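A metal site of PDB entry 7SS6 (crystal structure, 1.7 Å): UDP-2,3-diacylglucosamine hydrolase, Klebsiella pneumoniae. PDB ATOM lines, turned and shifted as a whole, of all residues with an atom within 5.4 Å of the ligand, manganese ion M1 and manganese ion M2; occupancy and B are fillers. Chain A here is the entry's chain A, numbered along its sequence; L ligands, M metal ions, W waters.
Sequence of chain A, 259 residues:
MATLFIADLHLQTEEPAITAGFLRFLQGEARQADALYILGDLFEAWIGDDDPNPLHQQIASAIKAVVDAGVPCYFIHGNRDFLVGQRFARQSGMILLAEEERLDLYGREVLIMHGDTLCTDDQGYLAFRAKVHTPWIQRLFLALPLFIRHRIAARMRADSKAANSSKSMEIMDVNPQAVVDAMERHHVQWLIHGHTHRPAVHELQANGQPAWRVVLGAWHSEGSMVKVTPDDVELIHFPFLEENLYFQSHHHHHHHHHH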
ATOM      1  N   ASP A   8       6.632 -18.141  19.292  1.00  0.00           N
ATOM      2  CA  ASP A   8       6.472 -16.718  19.504  1.00  0.00           C
ATOM      3  C   ASP A   8       6.306 -16.361  20.976  1.00  0.00           C
ATOM      4  O   ASP A   8       5.471 -15.537  21.350  1.00  0.00           O
ATOM      5  CB  ASP A   8       5.298 -16.211  18.668  1.00  0.00           C
ATOM      6  CG  ASP A   8       5.564 -16.385  17.185  1.00  0.00           C
ATOM      7  OD1 ASP A   8       6.529 -15.768  16.717  1.00  0.00           O
ATOM      8  OD2 ASP A   8       4.831 -17.117  16.499  1.00  0.00           O
ATOM      9  N   HIS A  10       9.060 -15.117  22.576  1.00  0.00           N
ATOM     10  CA  HIS A  10       9.952 -13.945  22.620  1.00  0.00           C
ATOM     11  C   HIS A  10      10.499 -13.723  24.030  1.00  0.00           C
ATOM     12  O   HIS A  10      10.461 -12.616  24.565  1.00  0.00           O
ATOM     13  CB  HIS A  10       9.224 -12.691  22.112  1.00  0.00           C
ATOM     14  CG  HIS A  10       8.439 -12.920  20.863  1.00  0.00           C
ATOM     15  ND1 HIS A  10       7.066 -12.944  20.836  1.00  0.00           N
ATOM     16  CD2 HIS A  10       8.845 -13.150  19.588  1.00  0.00           C
ATOM     17  CE1 HIS A  10       6.648 -13.186  19.610  1.00  0.00           C
ATOM     18  NE2 HIS A  10       7.713 -13.321  18.835  1.00  0.00           N
ATOM     19  N   ASP A  41      11.030 -18.457  17.398  1.00  0.00           N
ATOM     20  CA  ASP A  41      10.865 -17.255  18.232  1.00  0.00           C
ATOM     21  C   ASP A  41      10.584 -17.640  19.679  1.00  0.00           C
ATOM     22  O   ASP A  41       9.771 -17.029  20.383  1.00  0.00           O
ATOM     23  CB  ASP A  41       9.772 -16.334  17.676  1.00  0.00           C
ATOM     24  CG  ASP A  41      10.177 -15.641  16.384  1.00  0.00           C
ATOM     25  OD1 ASP A  41      11.322 -15.815  15.931  1.00  0.00           O
ATOM     26  OD2 ASP A  41       9.338 -14.917  15.845  1.00  0.00           O
ATOM     27  N   GLU A  44      13.539 -13.704  22.242  1.00  0.00           N
ATOM     28  CA  GLU A  44      13.402 -12.447  21.512  1.00  0.00           C
ATOM     29  C   GLU A  44      14.647 -12.125  20.707  1.00  0.00           C
ATOM     30  O   GLU A  44      14.576 -11.395  19.706  1.00  0.00           O
ATOM     31  CB  GLU A  44      13.092 -11.318  22.507  1.00  0.00           C
ATOM     32  CG  GLU A  44      13.135  -9.884  21.917  1.00  0.00           C
ATOM     33  CD  GLU A  44      12.033  -9.554  20.919  1.00  0.00           C
ATOM     34  OE1 GLU A  44      11.238 -10.432  20.551  1.00  0.00           O
ATOM     35  OE2 GLU A  44      11.987  -8.381  20.473  1.00  0.00           O
ATOM     36  N   ALA A  45      15.793 -12.669  21.112  1.00  0.00           N
ATOM     37  CA  ALA A  45      17.047 -12.436  20.421  1.00  0.00           C
ATOM     38  C   ALA A  45      17.962 -13.626  20.665  1.00  0.00           C
ATOM     39  O   ALA A  45      17.828 -14.316  21.673  1.00  0.00           O
ATOM     40  CB  ALA A  45      17.713 -11.139  20.921  1.00  0.00           C
ATOM     41  N   TRP A  46      18.901 -13.858  19.741  1.00  0.00           N
ATOM     42  CA  TRP A  46      19.952 -14.840  19.967  1.00  0.00           C
ATOM     43  C   TRP A  46      21.175 -14.400  19.174  1.00  0.00           C
ATOM     44  O   TRP A  46      21.073 -14.119  17.986  1.00  0.00           O
ATOM     45  CB  TRP A  46      19.542 -16.244  19.502  1.00  0.00           C
ATOM     46  CG  TRP A  46      20.314 -17.381  20.161  1.00  0.00           C
ATOM     47  CD1 TRP A  46      21.393 -18.060  19.657  1.00  0.00           C
ATOM     48  CD2 TRP A  46      20.024 -17.973  21.438  1.00  0.00           C
ATOM     49  NE1 TRP A  46      21.793 -19.044  20.560  1.00  0.00           N
ATOM     50  CE2 TRP A  46      20.969 -18.995  21.656  1.00  0.00           C
ATOM     51  CE3 TRP A  46      19.052 -17.724  22.418  1.00  0.00           C
ATOM     52  CZ2 TRP A  46      20.949 -19.798  22.813  1.00  0.00           C
ATOM     53  CZ3 TRP A  46      19.045 -18.522  23.576  1.00  0.00           C
ATOM     54  CH2 TRP A  46      19.986 -19.542  23.748  1.00  0.00           C
ATOM     55  N   ILE A  47      22.327 -14.348  19.846  1.00  0.00           N
ATOM     56  CA  ILE A  47      23.578 -13.987  19.178  1.00  0.00           C
ATOM     57  C   ILE A  47      24.592 -15.120  19.229  1.00  0.00           C
ATOM     58  O   ILE A  47      25.742 -14.934  18.833  1.00  0.00           O
ATOM     59  CB  ILE A  47      24.173 -12.678  19.751  1.00  0.00           C
ATOM     60  CG1 ILE A  47      24.491 -12.815  21.250  1.00  0.00           C
ATOM     61  CG2 ILE A  47      23.243 -11.501  19.469  1.00  0.00           C
ATOM     62  CD1 ILE A  47      25.214 -11.608  21.827  1.00  0.00           C
ATOM     63  N   GLY A  78      13.041 -19.607  14.603  1.00  0.00           N
ATOM     64  CA  GLY A  78      12.329 -18.414  14.172  1.00  0.00           C
ATOM     65  C   GLY A  78      13.293 -17.403  13.586  1.00  0.00           C
ATOM     66  O   GLY A  78      14.505 -17.603  13.552  1.00  0.00           O
ATOM     67  N   ASN A  79      12.739 -16.283  13.131  1.00  0.00           N
ATOM     68  CA  ASN A  79      13.576 -15.198  12.652  1.00  0.00           C
ATOM     69  C   ASN A  79      14.267 -14.451  13.788  1.00  0.00           C
ATOM     70  O   ASN A  79      15.285 -13.799  13.550  1.00  0.00           O
ATOM     71  CB  ASN A  79      12.750 -14.223  11.820  1.00  0.00           C
ATOM     72  CG  ASN A  79      11.593 -13.655  12.589  1.00  0.00           C
ATOM     73  OD1 ASN A  79      10.638 -14.369  12.910  1.00  0.00           O
ATOM     74  ND2 ASN A  79      11.641 -12.362  12.878  1.00  0.00           N
ATOM     75  N   ARG A  80      13.737 -14.528  15.021  1.00  0.00           N
ATOM     76  CA  ARG A  80      14.426 -13.892  16.130  1.00  0.00           C
ATOM     77  C   ARG A  80      15.587 -14.742  16.635  1.00  0.00           C
ATOM     78  O   ARG A  80      16.600 -14.190  17.107  1.00  0.00           O
ATOM     79  CB  ARG A  80      13.464 -13.607  17.293  1.00  0.00           C
ATOM     80  CG  ARG A  80      12.222 -12.796  16.944  1.00  0.00           C
ATOM     81  CD  ARG A  80      12.592 -11.414  16.383  1.00  0.00           C
ATOM     82  NE  ARG A  80      13.332 -10.622  17.357  1.00  0.00           N
ATOM     83  CZ  ARG A  80      13.503  -9.313  17.274  1.00  0.00           C
ATOM     84  NH1 ARG A  80      12.943  -8.597  16.307  1.00  0.00           N
ATOM     85  NH2 ARG A  80      14.252  -8.692  18.180  1.00  0.00           N
ATOM     86  N   PHE A  82      17.299 -17.536  15.022  1.00  0.00           N
ATOM     87  CA  PHE A  82      17.859 -18.444  14.030  1.00  0.00           C
ATOM     88  C   PHE A  82      19.294 -18.874  14.353  1.00  0.00           C
ATOM     89  O   PHE A  82      19.773 -19.856  13.775  1.00  0.00           O
ATOM     90  CB  PHE A  82      17.826 -17.810  12.622  1.00  0.00           C
ATOM     91  CG  PHE A  82      18.599 -16.526  12.486  1.00  0.00           C
ATOM     92  CD1 PHE A  82      18.000 -15.302  12.780  1.00  0.00           C
ATOM     93  CD2 PHE A  82      19.929 -16.534  12.072  1.00  0.00           C
ATOM     94  CE1 PHE A  82      18.714 -14.104  12.656  1.00  0.00           C
ATOM     95  CE2 PHE A  82      20.638 -15.344  11.953  1.00  0.00           C
ATOM     96  CZ  PHE A  82      20.028 -14.134  12.255  1.00  0.00           C
ATOM     97  N   LEU A  83      19.959 -18.216  15.290  1.00  0.00           N
ATOM     98  CA  LEU A  83      21.313 -18.638  15.643  1.00  0.00           C
ATOM     99  C   LEU A  83      21.354 -19.676  16.756  1.00  0.00           C
ATOM    100  O   LEU A  83      22.458 -20.067  17.161  1.00  0.00           O
ATOM    101  CB  LEU A  83      22.167 -17.421  16.053  1.00  0.00           C
ATOM    102  CG  LEU A  83      22.511 -16.455  14.912  1.00  0.00           C
ATOM    103  CD1 LEU A  83      23.344 -15.307  15.432  1.00  0.00           C
ATOM    104  CD2 LEU A  83      23.261 -17.194  13.790  1.00  0.00           C
ATOM    105  N   HIS A 114       8.051 -22.191  11.041  1.00  0.00           N
ATOM    106  CA  HIS A 114       7.868 -20.965  11.802  1.00  0.00           C
ATOM    107  C   HIS A 114       6.807 -20.088  11.144  1.00  0.00           C
ATOM    108  O   HIS A 114       5.958 -19.495  11.821  1.00  0.00           O
ATOM    109  CB  HIS A 114       9.167 -20.177  11.940  1.00  0.00           C
ATOM    110  CG  HIS A 114       9.010 -18.925  12.731  1.00  0.00           C
ATOM    111  ND1 HIS A 114       8.527 -18.919  14.021  1.00  0.00           N
ATOM    112  CD2 HIS A 114       9.200 -17.616  12.401  1.00  0.00           C
ATOM    113  CE1 HIS A 114       8.463 -17.681  14.469  1.00  0.00           C
ATOM    114  NE2 HIS A 114       8.865 -16.869  13.505  1.00  0.00           N
ATOM    115  N   ASP A 116       7.575 -17.558   8.677  1.00  0.00           N
ATOM    116  CA  ASP A 116       8.039 -16.344   7.996  1.00  0.00           C
ATOM    117  C   ASP A 116       8.333 -16.575   6.520  1.00  0.00           C
ATOM    118  O   ASP A 116       8.217 -15.641   5.710  1.00  0.00           O
ATOM    119  CB  ASP A 116       9.284 -15.770   8.686  1.00  0.00           C
ATOM    120  CG  ASP A 116      10.434 -16.762   8.765  1.00  0.00           C
ATOM    121  OD1 ASP A 116      10.228 -17.925   9.182  1.00  0.00           O
ATOM    122  OD2 ASP A 116      11.571 -16.356   8.446  1.00  0.00           O
ATOM    123  N   TYR A 125      12.192  -8.387   3.503  1.00  0.00           N
ATOM    124  CA  TYR A 125      12.486  -9.291   4.614  1.00  0.00           C
ATOM    125  C   TYR A 125      13.146 -10.573   4.115  1.00  0.00           C
ATOM    126  O   TYR A 125      14.161 -11.021   4.661  1.00  0.00           O
ATOM    127  CB  TYR A 125      11.211  -9.610   5.389  1.00  0.00           C
ATOM    128  CG  TYR A 125      11.461 -10.765   6.328  1.00  0.00           C
ATOM    129  CD1 TYR A 125      12.308 -10.608   7.400  1.00  0.00           C
ATOM    130  CD2 TYR A 125      10.913 -12.006   6.080  1.00  0.00           C
ATOM    131  CE1 TYR A 125      12.572 -11.662   8.252  1.00  0.00           C
ATOM    132  CE2 TYR A 125      11.174 -13.074   6.931  1.00  0.00           C
ATOM    133  CZ  TYR A 125      12.010 -12.887   8.014  1.00  0.00           C
ATOM    134  OH  TYR A 125      12.281 -13.920   8.865  1.00  0.00           O
ATOM    135  N   PHE A 128      16.895 -10.112   3.323  1.00  0.00           N
ATOM    136  CA  PHE A 128      17.653 -10.098   4.572  1.00  0.00           C
ATOM    137  C   PHE A 128      17.705 -11.490   5.206  1.00  0.00           C
ATOM    138  O   PHE A 128      18.747 -11.918   5.703  1.00  0.00           O
ATOM    139  CB  PHE A 128      17.019  -9.108   5.544  1.00  0.00           C
ATOM    140  CG  PHE A 128      17.509  -9.242   6.957  1.00  0.00           C
ATOM    141  CD1 PHE A 128      18.764  -8.790   7.324  1.00  0.00           C
ATOM    142  CD2 PHE A 128      16.702  -9.843   7.928  1.00  0.00           C
ATOM    143  CE1 PHE A 128      19.202  -8.924   8.630  1.00  0.00           C
ATOM    144  CE2 PHE A 128      17.143  -9.984   9.228  1.00  0.00           C
ATOM    145  CZ  PHE A 128      18.396  -9.522   9.585  1.00  0.00           C
ATOM    146  N   VAL A 132      21.206 -13.625   6.367  1.00  0.00           N
ATOM    147  CA  VAL A 132      21.574 -14.143   7.681  1.00  0.00           C
ATOM    148  C   VAL A 132      21.454 -15.653   7.785  1.00  0.00           C
ATOM    149  O   VAL A 132      21.836 -16.226   8.802  1.00  0.00           O
ATOM    150  CB  VAL A 132      20.763 -13.509   8.831  1.00  0.00           C
ATOM    151  CG1 VAL A 132      21.006 -11.999   8.892  1.00  0.00           C
ATOM    152  CG2 VAL A 132      19.263 -13.843   8.707  1.00  0.00           C
ATOM    153  N   ILE A 137      28.134 -16.186   6.275  1.00  0.00           N
ATOM    154  CA  ILE A 137      27.783 -14.996   7.028  1.00  0.00           C
ATOM    155  C   ILE A 137      27.538 -15.340   8.495  1.00  0.00           C
ATOM    156  O   ILE A 137      28.017 -14.643   9.390  1.00  0.00           O
ATOM    157  CB  ILE A 137      26.583 -14.293   6.371  1.00  0.00           C
ATOM    158  CG1 ILE A 137      26.960 -13.809   4.974  1.00  0.00           C
ATOM    159  CG2 ILE A 137      26.098 -13.129   7.219  1.00  0.00           C
ATOM    160  CD1 ILE A 137      25.856 -13.084   4.239  1.00  0.00           C
ATOM    161  N   GLN A 138      26.791 -16.423   8.770  1.00  0.00           N
ATOM    162  CA  GLN A 138      26.599 -16.835  10.165  1.00  0.00           C
ATOM    163  C   GLN A 138      27.927 -17.134  10.847  1.00  0.00           C
ATOM    164  O   GLN A 138      28.136 -16.742  12.005  1.00  0.00           O
ATOM    165  CB  GLN A 138      25.696 -18.065  10.240  1.00  0.00           C
ATOM    166  CG  GLN A 138      24.280 -17.811   9.830  1.00  0.00           C
ATOM    167  CD  GLN A 138      23.392 -18.946  10.235  1.00  0.00           C
ATOM    168  OE1 GLN A 138      23.870 -19.957  10.756  1.00  0.00           O
ATOM    169  NE2 GLN A 138      22.091 -18.798  10.011  1.00  0.00           N
ATOM    170  N   PHE A 141      29.715 -13.870  11.727  1.00  0.00           N
ATOM    171  CA  PHE A 141      29.090 -13.184  12.864  1.00  0.00           C
ATOM    172  C   PHE A 141      29.452 -13.867  14.171  1.00  0.00           C
ATOM    173  O   PHE A 141      29.838 -13.221  15.144  1.00  0.00           O
ATOM    174  CB  PHE A 141      27.567 -13.139  12.684  1.00  0.00           C
ATOM    175  CG  PHE A 141      26.846 -12.484  13.838  1.00  0.00           C
ATOM    176  CD1 PHE A 141      26.713 -11.103  13.901  1.00  0.00           C
ATOM    177  CD2 PHE A 141      26.287 -13.250  14.850  1.00  0.00           C
ATOM    178  CE1 PHE A 141      26.030 -10.507  14.955  1.00  0.00           C
ATOM    179  CE2 PHE A 141      25.630 -12.645  15.907  1.00  0.00           C
ATOM    180  CZ  PHE A 141      25.493 -11.292  15.965  1.00  0.00           C
ATOM    181  N   ILE A 152      26.074  -5.105  18.269  1.00  0.00           N
ATOM    182  CA  ILE A 152      25.435  -5.139  16.946  1.00  0.00           C
ATOM    183  C   ILE A 152      23.943  -5.414  17.111  1.00  0.00           C
ATOM    184  O   ILE A 152      23.088  -4.709  16.568  1.00  0.00           O
ATOM    185  CB  ILE A 152      26.080  -6.194  16.039  1.00  0.00           C
ATOM    186  CG1 ILE A 152      27.481  -5.755  15.588  1.00  0.00           C
ATOM    187  CG2 ILE A 152      25.191  -6.495  14.839  1.00  0.00           C
ATOM    188  CD1 ILE A 152      28.254  -6.877  14.921  1.00  0.00           C
ATOM    189  N   ALA A 153      23.623  -6.436  17.918  1.00  0.00           N
ATOM    190  CA  ALA A 153      22.229  -6.850  18.080  1.00  0.00           C
ATOM    191  C   ALA A 153      21.406  -5.757  18.753  1.00  0.00           C
ATOM    192  O   ALA A 153      20.268  -5.498  18.340  1.00  0.00           O
ATOM    193  CB  ALA A 153      22.171  -8.147  18.878  1.00  0.00           C
ATOM    194  N   ALA A 154      21.962  -5.114  19.785  1.00  0.00           N
ATOM    195  CA  ALA A 154      21.215  -4.066  20.474  1.00  0.00           C
ATOM    196  C   ALA A 154      20.949  -2.889  19.550  1.00  0.00           C
ATOM    197  O   ALA A 154      19.847  -2.310  19.569  1.00  0.00           O
ATOM    198  CB  ALA A 154      21.967  -3.606  21.726  1.00  0.00           C
ATOM    199  N   MET A 156      20.729  -3.076  16.238  1.00  0.00           N
ATOM    200  CA  MET A 156      19.761  -3.559  15.256  1.00  0.00           C
ATOM    201  C   MET A 156      18.347  -3.559  15.827  1.00  0.00           C
ATOM    202  O   MET A 156      17.383  -3.181  15.139  1.00  0.00           O
ATOM    203  CB  MET A 156      20.183  -4.969  14.832  1.00  0.00           C
ATOM    204  CG  MET A 156      21.456  -4.963  14.014  1.00  0.00           C
ATOM    205  SD  MET A 156      21.737  -6.417  12.992  1.00  0.00           S
ATOM    206  CE  MET A 156      20.090  -6.783  12.397  1.00  0.00           C
ATOM    207  N   ARG A 157      18.198  -3.994  17.077  1.00  0.00           N
ATOM    208  CA  ARG A 157      16.889  -3.969  17.723  1.00  0.00           C
ATOM    209  C   ARG A 157      16.421  -2.535  17.952  1.00  0.00           C
ATOM    210  O   ARG A 157      15.238  -2.219  17.739  1.00  0.00           O
ATOM    211  CB  ARG A 157      16.922  -4.744  19.033  1.00  0.00           C
ATOM    212  CG  ARG A 157      17.105  -6.258  18.857  1.00  0.00           C
ATOM    213  CD  ARG A 157      16.854  -7.000  20.159  1.00  0.00           C
ATOM    214  NE  ARG A 157      17.756  -6.558  21.221  1.00  0.00           N
ATOM    215  CZ  ARG A 157      18.960  -7.076  21.443  1.00  0.00           C
ATOM    216  NH1 ARG A 157      19.433  -8.073  20.722  1.00  0.00           N
ATOM    217  NH2 ARG A 157      19.703  -6.579  22.432  1.00  0.00           N
ATOM    218  N   SER A 160      15.218  -1.234  14.606  1.00  0.00           N
ATOM    219  CA  SER A 160      13.982  -1.805  14.086  1.00  0.00           C
ATOM    220  C   SER A 160      12.752  -1.303  14.842  1.00  0.00           C
ATOM    221  O   SER A 160      11.654  -1.262  14.277  1.00  0.00           O
ATOM    222  CB  SER A 160      14.037  -3.326  14.131  1.00  0.00           C
ATOM    223  OG  SER A 160      14.841  -3.839  13.082  1.00  0.00           O
ATOM    224  N   ILE A 171       3.089  -6.899  11.442  1.00  0.00           N
ATOM    225  CA  ILE A 171       3.760  -8.013  10.782  1.00  0.00           C
ATOM    226  C   ILE A 171       3.015  -8.381   9.507  1.00  0.00           C
ATOM    227  O   ILE A 171       1.793  -8.598   9.520  1.00  0.00           O
ATOM    228  CB  ILE A 171       3.874  -9.214  11.735  1.00  0.00           C
ATOM    229  CG1 ILE A 171       4.388  -8.755  13.115  1.00  0.00           C
ATOM    230  CG2 ILE A 171       4.695 -10.354  11.118  1.00  0.00           C
ATOM    231  CD1 ILE A 171       4.477  -9.865  14.143  1.00  0.00           C
ATOM    232  N   HIS A 195       4.809 -16.950  13.797  1.00  0.00           N
ATOM    233  CA  HIS A 195       5.347 -15.754  13.148  1.00  0.00           C
ATOM    234  C   HIS A 195       4.360 -14.606  12.954  1.00  0.00           C
ATOM    235  O   HIS A 195       4.709 -13.452  13.254  1.00  0.00           O
ATOM    236  CB  HIS A 195       5.970 -16.087  11.802  1.00  0.00           C
ATOM    237  CG  HIS A 195       6.662 -14.905  11.176  1.00  0.00           C
ATOM    238  ND1 HIS A 195       7.803 -14.342  11.704  1.00  0.00           N
ATOM    239  CD2 HIS A 195       6.360 -14.163  10.081  1.00  0.00           C
ATOM    240  CE1 HIS A 195       8.183 -13.312  10.958  1.00  0.00           C
ATOM    241  NE2 HIS A 195       7.316 -13.189   9.963  1.00  0.00           N
ATOM    242  N   THR A 196       3.160 -14.871  12.441  1.00  0.00           N
ATOM    243  CA  THR A 196       2.268 -13.763  12.110  1.00  0.00           C
ATOM    244  C   THR A 196       1.546 -13.199  13.318  1.00  0.00           C
ATOM    245  O   THR A 196       0.919 -12.142  13.215  1.00  0.00           O
ATOM    246  CB  THR A 196       1.254 -14.189  11.057  1.00  0.00           C
ATOM    247  OG1 THR A 196       0.423 -15.242  11.595  1.00  0.00           O
ATOM    248  CG2 THR A 196       1.972 -14.691   9.791  1.00  0.00           C
ATOM    249  N   HIS A 197       1.590 -13.887  14.468  1.00  0.00           N
ATOM    250  CA  HIS A 197       0.998 -13.417  15.717  1.00  0.00           C
ATOM    251  C   HIS A 197      -0.509 -13.202  15.587  1.00  0.00           C
ATOM    252  O   HIS A 197      -1.082 -12.332  16.254  1.00  0.00           O
ATOM    253  CB  HIS A 197       1.673 -12.140  16.196  1.00  0.00           C
ATOM    254  CG  HIS A 197       3.138 -12.304  16.517  1.00  0.00           C
ATOM    255  ND1 HIS A 197       3.881 -11.287  17.076  1.00  0.00           N
ATOM    256  CD2 HIS A 197       3.972 -13.355  16.376  1.00  0.00           C
ATOM    257  CE1 HIS A 197       5.123 -11.717  17.263  1.00  0.00           C
ATOM    258  NE2 HIS A 197       5.217 -12.954  16.827  1.00  0.00           N
HETATM  259  C1  LIG L   1      16.807 -10.841  15.486  1.00  0.00           C
HETATM  260  C2  LIG L   1      15.585  -9.120  14.336  1.00  0.00           C
HETATM  261  C3  LIG L   1      17.377  -8.470  15.791  1.00  0.00           C
HETATM  262  C4  LIG L   1      13.473  -9.187  12.853  1.00  0.00           C
HETATM  263  C5  LIG L   1      11.397  -9.115  11.416  1.00  0.00           C
HETATM  264  C6  LIG L   1       9.034  -9.902  11.993  1.00  0.00           C
HETATM  265  C7  LIG L   1       8.181 -11.517  13.723  1.00  0.00           C
HETATM  266  C8  LIG L   1      23.175 -12.249  12.577  1.00  0.00           C
HETATM  267  C9  LIG L   1      22.914 -10.971  13.019  1.00  0.00           C
HETATM  268  C10 LIG L   1      22.128  -9.623  14.987  1.00  0.00           C
HETATM  269  C11 LIG L   1      20.718  -9.332  15.477  1.00  0.00           C
HETATM  270  C12 LIG L   1      20.241 -11.684  15.447  1.00  0.00           C
HETATM  271  C13 LIG L   1      21.602 -12.008  14.867  1.00  0.00           C
HETATM  272  C14 LIG L   1      17.560  -9.812  16.053  1.00  0.00           C
HETATM  273  C15 LIG L   1      15.785 -10.491  14.616  1.00  0.00           C
HETATM  274  C16 LIG L   1      16.352  -8.110  14.911  1.00  0.00           C
HETATM  275  C17 LIG L   1      15.882  -6.742  14.422  1.00  0.00           C
HETATM  276  C18 LIG L   1      14.805  -7.047  13.403  1.00  0.00           C
HETATM  277  C19 LIG L   1      10.338  -9.275  12.546  1.00  0.00           C
HETATM  278  C20 LIG L   1       7.998 -10.123  13.118  1.00  0.00           C
HETATM  279  C21 LIG L   1      23.450  -9.842  12.416  1.00  0.00           C
HETATM  280  C22 LIG L   1      24.261 -10.019  11.319  1.00  0.00           C
HETATM  281  C23 LIG L   1      24.535 -11.283  10.827  1.00  0.00           C
HETATM  282  C24 LIG L   1      23.969 -12.399  11.461  1.00  0.00           C
HETATM  283  C25 LIG L   1      24.847  -8.770  10.657  1.00  0.00           C
HETATM  284  F1  LIG L   1      23.811  -7.965  10.315  1.00  0.00           F
HETATM  285  F2  LIG L   1      25.539  -9.153   9.555  1.00  0.00           F
HETATM  286  F3  LIG L   1      25.649  -8.120  11.517  1.00  0.00           F
HETATM  287  N1  LIG L   1      22.068 -10.810  14.160  1.00  0.00           N
HETATM  288  N2  LIG L   1      20.282 -10.485  16.270  1.00  0.00           N
HETATM  289  N3  LIG L   1      14.568  -8.480  13.474  1.00  0.00           N
HETATM  290  N4  LIG L   1      12.524  -8.415  12.041  1.00  0.00           N
HETATM  291  N5  LIG L   1       7.031 -12.341  14.061  1.00  0.00           N
HETATM  292  O1  LIG L   1      19.048  -9.153  18.137  1.00  0.00           O
HETATM  293  O2  LIG L   1      18.566 -11.501  17.861  1.00  0.00           O
HETATM  294  O3  LIG L   1      13.376 -10.356  12.982  1.00  0.00           O
HETATM  295  O4  LIG L   1       9.261 -11.983  13.930  1.00  0.00           O
HETATM  296  O5  LIG L   1       7.326 -13.598  14.617  1.00  0.00           O
HETATM  297  S1  LIG L   1      18.883 -10.233  17.183  1.00  0.00           S
HETATM  298 CL1  LIG L   1      24.295 -14.023  10.866  1.00  0.00          CL
HETATM  299 MN    MN M   1       8.863 -14.619  13.753  1.00  0.00          MN
HETATM  300 MN    MN M   2       7.319 -13.880  16.691  1.00  0.00          MN
HETATM  301  O   HOH W   1       8.621 -11.842  16.474  1.00  0.00           O
HETATM  302  O   HOH W   2       9.652  -9.275  15.862  1.00  0.00           O
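The guanidinium group (NH1) of Arg 157 sits at hydrogen-bond distance from an oxygen (O1) of the ligand, at 2.8 Å.
The backbone NH (N) of Trp 46 lies within hydrogen-bond range of an oxygen (O2) of the ligand.
A nitrogen (N5) of the ligand is in hydrogen-bond range of the backbone carbonyl oxygen (O) of His 195 (2.7 Å).
The side-chain carboxylate of Asp 8 is in hydrogen-bond range of the backbone NH of His 195 (2.7 Å).
O of Met 156 is in hydrogen-bond range of OG of Ser 160 (3.3 Å).
The guanidinium group of Arg 80 lies within salt-bridge range of the side-chain carboxylate of Glu 44 (3.2 Å).
The backbone NH of Arg 80 is in hydrogen-bond range of the side-chain carboxylate of Asp 41, at 2.9 Å.
NE2 of Gln 138 sits at hydrogen-bond distance from O of Val 132, at 2.9 Å.
The guanidinium group (NH1) of Arg 80 sits close to a nitrogen (N3) of the ligand.
SD of Met 156 sits close to F1 of the ligand, at 3.7 Å.
Ala 45 touches the ligand.
CZ of Phe 82 touches C8 of the ligand (3.7 Å).
Leu 83 touches the ligand.
Val 132 touches the ligand.
CA of Gln 138 touches CL1 of the ligand, 3.7 Å away.
Phe 141 touches the ligand (CE1 to C21, 3.7 Å).
CG2 of Ile 152 touches F3 of the ligand (3.7 Å).
CB of Ala 153 touches O1 of the ligand, 3.4 Å away.
OG of Ser 160 touches C18 of the ligand, at 3.2 Å.
Ile 171 touches the ligand (CD1 to N5, 3.6 Å).
Hydrophobic or aromatic side chains within 4 Å of the ligand: Ala 45, Phe 82, Leu 83, Val 132, Phe 141, Ile 152, Ala 153, Met 156, Ile 171, His 195 and His 197.
Within 4 Å of the ligand: Asp 8, Asp 41, Ala 45, Trp 46, Asn 79, Arg 80, Phe 82, Leu 83, His 114, Val 132, Gln 138, Phe 141, Ile 152, Ala 153, Met 156, Arg 157, Ser 160, Ile 171, His 195 and His 197.
The nearest printed residue that does not touch the ligand is Ile 137 (4.1 Å).
Of the 30 residues printed, 5 come within 4 Å of manganese ion M1.
Along chain A the residues within 4 Å of manganese ion M1 span positions 8 to 195.
Four residues have an atom within 4 Å of manganese ion M2: Asp 8, His 10, Asp 41 and His 197.
The nearest printed residue that does not touch manganese ion M2 is His 195 (4.3 Å).
Manganese ion M1 is bound by the side-chain amide oxygen of Asn 79 (2.0 Å), an oxygen (O5) of the ligand (2.0 Å), the side-chain carboxylate of Asp 41 (2.2 Å), a ring nitrogen (NE2) of His 114 (2.3 Å), a ring nitrogen (ND1) of His 195 (2.3 Å) and an oxygen (O4) of the ligand (2.7 Å).
Manganese ion M1 has six donor atoms within binding distance.
Manganese ion M2 is bound by the side-chain carboxylate of Asp 8 (2.0 Å), an oxygen (O5) of the ligand (2.1 Å), a ring nitrogen (NE2) of His 10 (2.3 Å), a ring nitrogen (NE2) of His 197 (2.3 Å), the side-chain carboxylate of Asp 41 (2.4 Å) and water W1 (2.4 Å).
Manganese ion M2 has six donor atoms within binding distance.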
